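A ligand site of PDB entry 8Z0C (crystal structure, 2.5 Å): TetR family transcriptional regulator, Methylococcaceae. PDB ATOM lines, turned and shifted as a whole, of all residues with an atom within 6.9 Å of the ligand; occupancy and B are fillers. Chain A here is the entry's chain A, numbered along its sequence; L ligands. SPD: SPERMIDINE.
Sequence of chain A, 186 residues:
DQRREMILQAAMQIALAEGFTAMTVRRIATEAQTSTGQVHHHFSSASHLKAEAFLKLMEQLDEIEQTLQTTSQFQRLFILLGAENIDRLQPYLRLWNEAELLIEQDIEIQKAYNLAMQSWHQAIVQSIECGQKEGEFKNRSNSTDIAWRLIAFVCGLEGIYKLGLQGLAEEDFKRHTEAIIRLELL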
ATOM      1  N   LEU A  61      15.343   4.655 -11.331  1.00  0.00           N
ATOM      2  CA  LEU A  61      14.555   5.692 -11.995  1.00  0.00           C
ATOM      3  C   LEU A  61      14.515   6.963 -11.157  1.00  0.00           C
ATOM      4  O   LEU A  61      14.819   8.058 -11.647  1.00  0.00           O
ATOM      5  CB  LEU A  61      13.118   5.208 -12.236  1.00  0.00           C
ATOM      6  CG  LEU A  61      12.193   6.093 -13.076  1.00  0.00           C
ATOM      7  CD1 LEU A  61      12.883   6.605 -14.355  1.00  0.00           C
ATOM      8  CD2 LEU A  61      10.849   5.429 -13.355  1.00  0.00           C
ATOM      9  N   ASP A  62      14.125   6.818  -9.898  1.00  0.00           N
ATOM     10  CA  ASP A  62      13.819   7.981  -9.096  1.00  0.00           C
ATOM     11  C   ASP A  62      15.079   8.710  -8.637  1.00  0.00           C
ATOM     12  O   ASP A  62      14.988   9.888  -8.284  1.00  0.00           O
ATOM     13  CB  ASP A  62      12.934   7.576  -7.924  1.00  0.00           C
ATOM     14  CG  ASP A  62      13.722   7.201  -6.674  1.00  0.00           C
ATOM     15  OD1 ASP A  62      14.969   7.177  -6.700  1.00  0.00           O
ATOM     16  OD2 ASP A  62      13.074   6.921  -5.636  1.00  0.00           O
ATOM     17  N   GLU A  65      16.226  10.577 -11.220  1.00  0.00           N
ATOM     18  CA  GLU A  65      15.244  11.651 -11.249  1.00  0.00           C
ATOM     19  C   GLU A  65      15.606  12.795 -10.311  1.00  0.00           C
ATOM     20  O   GLU A  65      15.335  13.952 -10.619  1.00  0.00           O
ATOM     21  CB  GLU A  65      13.840  11.112 -10.923  1.00  0.00           C
ATOM     22  CG  GLU A  65      13.023  10.731 -12.161  1.00  0.00           C
ATOM     23  CD  GLU A  65      11.649  10.139 -11.827  1.00  0.00           C
ATOM     24  OE1 GLU A  65      11.413   9.763 -10.658  1.00  0.00           O
ATOM     25  OE2 GLU A  65      10.813  10.053 -12.764  1.00  0.00           O
ATOM     26  N   ILE A  79       7.658  16.011 -14.155  1.00  0.00           N
ATOM     27  CA  ILE A  79       8.495  14.870 -14.475  1.00  0.00           C
ATOM     28  C   ILE A  79       8.188  13.721 -13.518  1.00  0.00           C
ATOM     29  O   ILE A  79       8.039  12.578 -13.939  1.00  0.00           O
ATOM     30  CB  ILE A  79       9.974  15.280 -14.430  1.00  0.00           C
ATOM     31  CG1 ILE A  79      10.268  16.205 -15.624  1.00  0.00           C
ATOM     32  CG2 ILE A  79      10.869  14.046 -14.396  1.00  0.00           C
ATOM     33  CD1 ILE A  79      11.536  16.949 -15.496  1.00  0.00           C
ATOM     34  N   LEU A  80       8.068  14.012 -12.216  1.00  0.00           N
ATOM     35  CA  LEU A  80       7.789  12.975 -11.237  1.00  0.00           C
ATOM     36  C   LEU A  80       6.513  12.208 -11.566  1.00  0.00           C
ATOM     37  O   LEU A  80       6.460  10.987 -11.430  1.00  0.00           O
ATOM     38  CB  LEU A  80       7.668  13.574  -9.839  1.00  0.00           C
ATOM     39  CG  LEU A  80       8.924  13.799  -9.026  1.00  0.00           C
ATOM     40  CD1 LEU A  80       8.537  13.986  -7.566  1.00  0.00           C
ATOM     41  CD2 LEU A  80       9.917  12.628  -9.227  1.00  0.00           C
ATOM     42  N   LEU A  81       5.465  12.908 -11.992  1.00  0.00           N
ATOM     43  CA  LEU A  81       4.213  12.244 -12.334  1.00  0.00           C
ATOM     44  C   LEU A  81       4.363  11.316 -13.528  1.00  0.00           C
ATOM     45  O   LEU A  81       3.499  10.448 -13.740  1.00  0.00           O
ATOM     46  CB  LEU A  81       3.130  13.291 -12.578  1.00  0.00           C
ATOM     47  CG  LEU A  81       2.704  13.835 -11.224  1.00  0.00           C
ATOM     48  CD1 LEU A  81       1.850  15.076 -11.383  1.00  0.00           C
ATOM     49  CD2 LEU A  81       1.984  12.790 -10.394  1.00  0.00           C
ATOM     50  N   GLY A  82       5.455  11.441 -14.291  1.00  0.00           N
ATOM     51  CA  GLY A  82       5.617  10.773 -15.548  1.00  0.00           C
ATOM     52  C   GLY A  82       5.033  11.510 -16.715  1.00  0.00           C
ATOM     53  O   GLY A  82       5.116  11.025 -17.849  1.00  0.00           O
ATOM     54  N   ALA A  83       4.454  12.685 -16.479  1.00  0.00           N
ATOM     55  CA  ALA A  83       3.755  13.446 -17.505  1.00  0.00           C
ATOM     56  C   ALA A  83       4.691  14.087 -18.520  1.00  0.00           C
ATOM     57  O   ALA A  83       4.214  14.573 -19.558  1.00  0.00           O
ATOM     58  CB  ALA A  83       2.886  14.527 -16.854  1.00  0.00           C
ATOM     59  N   LEU A  89      14.314   8.165 -19.529  1.00  0.00           N
ATOM     60  CA  LEU A  89      13.532   7.383 -18.584  1.00  0.00           C
ATOM     61  C   LEU A  89      12.475   6.514 -19.253  1.00  0.00           C
ATOM     62  O   LEU A  89      11.965   5.589 -18.607  1.00  0.00           O
ATOM     63  CB  LEU A  89      12.874   8.316 -17.564  1.00  0.00           C
ATOM     64  CG  LEU A  89      13.825   9.314 -16.926  1.00  0.00           C
ATOM     65  CD1 LEU A  89      13.156  10.062 -15.753  1.00  0.00           C
ATOM     66  CD2 LEU A  89      15.110   8.628 -16.479  1.00  0.00           C
ATOM     67  N   LEU A  93       9.955   3.525 -17.512  1.00  0.00           N
ATOM     68  CA  LEU A  93       8.502   3.619 -17.495  1.00  0.00           C
ATOM     69  C   LEU A  93       7.855   2.480 -18.287  1.00  0.00           C
ATOM     70  O   LEU A  93       6.727   2.068 -17.973  1.00  0.00           O
ATOM     71  CB  LEU A  93       8.061   4.980 -18.053  1.00  0.00           C
ATOM     72  CG  LEU A  93       8.726   6.270 -17.525  1.00  0.00           C
ATOM     73  CD1 LEU A  93       8.554   7.441 -18.516  1.00  0.00           C
ATOM     74  CD2 LEU A  93       8.237   6.656 -16.136  1.00  0.00           C
ATOM     75  N   TRP A  96       7.750  -0.384 -15.811  1.00  0.00           N
ATOM     76  CA  TRP A  96       6.718  -0.111 -14.804  1.00  0.00           C
ATOM     77  C   TRP A  96       5.357  -0.604 -15.290  1.00  0.00           C
ATOM     78  O   TRP A  96       4.579  -1.167 -14.507  1.00  0.00           O
ATOM     79  CB  TRP A  96       6.664   1.386 -14.499  1.00  0.00           C
ATOM     80  CG  TRP A  96       5.992   1.768 -13.172  1.00  0.00           C
ATOM     81  CD1 TRP A  96       4.748   1.382 -12.728  1.00  0.00           C
ATOM     82  CD2 TRP A  96       6.521   2.629 -12.150  1.00  0.00           C
ATOM     83  NE1 TRP A  96       4.486   1.940 -11.488  1.00  0.00           N
ATOM     84  CE2 TRP A  96       5.553   2.705 -11.117  1.00  0.00           C
ATOM     85  CE3 TRP A  96       7.714   3.343 -12.016  1.00  0.00           C
ATOM     86  CZ2 TRP A  96       5.760   3.458  -9.970  1.00  0.00           C
ATOM     87  CZ3 TRP A  96       7.913   4.082 -10.862  1.00  0.00           C
ATOM     88  CH2 TRP A  96       6.944   4.136  -9.857  1.00  0.00           C
ATOM     89  N   ASN A  97       5.074  -0.428 -16.573  1.00  0.00           N
ATOM     90  CA  ASN A  97       3.757  -0.766 -17.090  1.00  0.00           C
ATOM     91  C   ASN A  97       3.631  -2.270 -17.307  1.00  0.00           C
ATOM     92  O   ASN A  97       2.580  -2.857 -16.994  1.00  0.00           O
ATOM     93  CB  ASN A  97       3.468  -0.002 -18.371  1.00  0.00           C
ATOM     94  CG  ASN A  97       3.421   1.511 -18.137  1.00  0.00           C
ATOM     95  OD1 ASN A  97       2.867   1.994 -17.144  1.00  0.00           O
ATOM     96  ND2 ASN A  97       4.015   2.270 -19.063  1.00  0.00           N
ATOM     97  N   GLU A 100       2.877  -3.651 -14.085  1.00  0.00           N
ATOM     98  CA  GLU A 100       1.514  -3.376 -13.635  1.00  0.00           C
ATOM     99  C   GLU A 100       0.558  -4.453 -14.116  1.00  0.00           C
ATOM    100  O   GLU A 100      -0.397  -4.808 -13.418  1.00  0.00           O
ATOM    101  CB  GLU A 100       1.060  -2.005 -14.133  1.00  0.00           C
ATOM    102  CG  GLU A 100      -0.306  -1.558 -13.600  1.00  0.00           C
ATOM    103  CD  GLU A 100      -0.799  -0.293 -14.257  1.00  0.00           C
ATOM    104  OE1 GLU A 100      -0.308   0.008 -15.363  1.00  0.00           O
ATOM    105  OE2 GLU A 100      -1.669   0.399 -13.655  1.00  0.00           O
ATOM    106  N   TYR A 113       5.777  -4.039  -7.189  1.00  0.00           N
ATOM    107  CA  TYR A 113       4.962  -2.957  -7.724  1.00  0.00           C
ATOM    108  C   TYR A 113       4.361  -2.114  -6.618  1.00  0.00           C
ATOM    109  O   TYR A 113       4.348  -0.876  -6.702  1.00  0.00           O
ATOM    110  CB  TYR A 113       3.848  -3.511  -8.595  1.00  0.00           C
ATOM    111  CG  TYR A 113       3.028  -2.479  -9.341  1.00  0.00           C
ATOM    112  CD1 TYR A 113       3.458  -1.949 -10.560  1.00  0.00           C
ATOM    113  CD2 TYR A 113       1.792  -2.056  -8.854  1.00  0.00           C
ATOM    114  CE1 TYR A 113       2.720  -1.067 -11.256  1.00  0.00           C
ATOM    115  CE2 TYR A 113       1.038  -1.135  -9.544  1.00  0.00           C
ATOM    116  CZ  TYR A 113       1.497  -0.649 -10.753  1.00  0.00           C
ATOM    117  OH  TYR A 113       0.740   0.284 -11.449  1.00  0.00           O
ATOM    118  N   MET A 117       5.091   1.915  -6.078  1.00  0.00           N
ATOM    119  CA  MET A 117       4.040   2.928  -6.017  1.00  0.00           C
ATOM    120  C   MET A 117       4.105   3.694  -4.707  1.00  0.00           C
ATOM    121  O   MET A 117       3.916   4.919  -4.684  1.00  0.00           O
ATOM    122  CB  MET A 117       2.675   2.284  -6.210  1.00  0.00           C
ATOM    123  CG  MET A 117       2.502   1.642  -7.563  1.00  0.00           C
ATOM    124  SD  MET A 117       1.915   2.762  -8.843  1.00  0.00           S
ATOM    125  CE  MET A 117       0.397   3.345  -8.103  1.00  0.00           C
ATOM    126  N   TRP A 120       6.777   6.233  -5.093  1.00  0.00           N
ATOM    127  CA  TRP A 120       6.263   7.253  -5.992  1.00  0.00           C
ATOM    128  C   TRP A 120       5.370   8.244  -5.249  1.00  0.00           C
ATOM    129  O   TRP A 120       5.501   9.461  -5.413  1.00  0.00           O
ATOM    130  CB  TRP A 120       5.480   6.596  -7.139  1.00  0.00           C
ATOM    131  CG  TRP A 120       5.097   7.530  -8.267  1.00  0.00           C
ATOM    132  CD1 TRP A 120       5.780   8.639  -8.668  1.00  0.00           C
ATOM    133  CD2 TRP A 120       3.958   7.414  -9.142  1.00  0.00           C
ATOM    134  NE1 TRP A 120       5.152   9.219  -9.739  1.00  0.00           N
ATOM    135  CE2 TRP A 120       4.017   8.497 -10.039  1.00  0.00           C
ATOM    136  CE3 TRP A 120       2.901   6.501  -9.254  1.00  0.00           C
ATOM    137  CZ2 TRP A 120       3.056   8.701 -11.043  1.00  0.00           C
ATOM    138  CZ3 TRP A 120       1.951   6.704 -10.250  1.00  0.00           C
ATOM    139  CH2 TRP A 120       2.032   7.802 -11.125  1.00  0.00           C
ATOM    140  N   VAL A 154      -3.146  10.956 -13.164  1.00  0.00           N
ATOM    141  CA  VAL A 154      -2.236  10.595 -14.252  1.00  0.00           C
ATOM    142  C   VAL A 154      -2.423   9.132 -14.625  1.00  0.00           C
ATOM    143  O   VAL A 154      -2.294   8.783 -15.797  1.00  0.00           O
ATOM    144  CB  VAL A 154      -0.769  10.916 -13.912  1.00  0.00           C
ATOM    145  CG1 VAL A 154      -0.558  12.432 -13.794  1.00  0.00           C
ATOM    146  CG2 VAL A 154      -0.326  10.188 -12.660  1.00  0.00           C
ATOM    147  N   CYS A 155      -2.769   8.264 -13.659  1.00  0.00           N
ATOM    148  CA  CYS A 155      -3.068   6.881 -14.015  1.00  0.00           C
ATOM    149  C   CYS A 155      -4.393   6.791 -14.745  1.00  0.00           C
ATOM    150  O   CYS A 155      -4.522   6.037 -15.725  1.00  0.00           O
ATOM    151  CB  CYS A 155      -3.083   5.988 -12.780  1.00  0.00           C
ATOM    152  SG  CYS A 155      -1.445   5.609 -12.061  1.00  0.00           S
ATOM    153  N   GLU A 158      -4.175   7.890 -18.473  1.00  0.00           N
ATOM    154  CA  GLU A 158      -3.637   6.814 -19.281  1.00  0.00           C
ATOM    155  C   GLU A 158      -4.727   5.805 -19.635  1.00  0.00           C
ATOM    156  O   GLU A 158      -4.955   5.501 -20.816  1.00  0.00           O
ATOM    157  CB  GLU A 158      -2.491   6.148 -18.517  1.00  0.00           C
ATOM    158  CG  GLU A 158      -1.163   6.869 -18.689  1.00  0.00           C
ATOM    159  CD  GLU A 158      -0.171   6.598 -17.552  1.00  0.00           C
ATOM    160  OE1 GLU A 158       0.384   7.600 -17.026  1.00  0.00           O
ATOM    161  OE2 GLU A 158       0.067   5.407 -17.218  1.00  0.00           O
HETATM  162  N1  SPD L   1       8.492   8.403 -11.828  1.00  0.00           N
HETATM  163  C2  SPD L   1       7.419   8.296 -12.799  1.00  0.00           C
HETATM  164  C3  SPD L   1       6.465   7.183 -12.366  1.00  0.00           C
HETATM  165  C4  SPD L   1       5.444   6.828 -13.435  1.00  0.00           C
HETATM  166  C5  SPD L   1       4.567   5.671 -13.010  1.00  0.00           C
HETATM  167  N6  SPD L   1       3.478   5.555 -13.960  1.00  0.00           N
HETATM  168  C7  SPD L   1       3.199   4.145 -14.210  1.00  0.00           C
HETATM  169  C8  SPD L   1       1.889   3.777 -13.510  1.00  0.00           C
HETATM  170  C9  SPD L   1       1.211   2.558 -14.118  1.00  0.00           C
HETATM  171  N10 SPD L   1       0.265   2.977 -15.149  1.00  0.00           N
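A nitrogen (N1) of the ligand lies within salt-bridge range of the side-chain carboxylate (OE2) of Glu 65 (3.0 Å).
OE1 of Glu 100 is in salt-bridge range of N10 of the ligand, 3.0 Å away.
N1 of the ligand lies close to O of Leu 80, at 3.3 Å.
A nitrogen (N10) of the ligand lies within salt-bridge range of the side-chain carboxylate of Glu 158 (3.2 Å).
N10 of the ligand lies within hydrogen-bond range of OD1 of Asn 97 (3.4 Å).
Merely in contact with the ligand: Trp 96 (3.5 Å), Tyr 113 (3.5 Å), Trp 120 (3.6 Å), Leu 93 (3.8 Å) and Gly 82 (3.997 Å).
Of the 19 residues printed, 10 come within 4 Å of the ligand.
OE2 of Glu 100 lies close to OH of Tyr 113.
O of Leu 80 lies within hydrogen-bond range of NE1 of Trp 120 (2.8 Å).
The side-chain amide nitrogen of Asn 97 sits at hydrogen-bond distance from the backbone carbonyl oxygen of Leu 93 (2.9 Å).
The indole nitrogen of Trp 96 sits at hydrogen-bond distance from the side-chain sulfur of Met 117 (3.8 Å).
The side-chain hydroxyl (OH) of Tyr 113 is in hydrogen-bond range of the side-chain sulfur (SD) of Met 117, 3.8 Å away.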
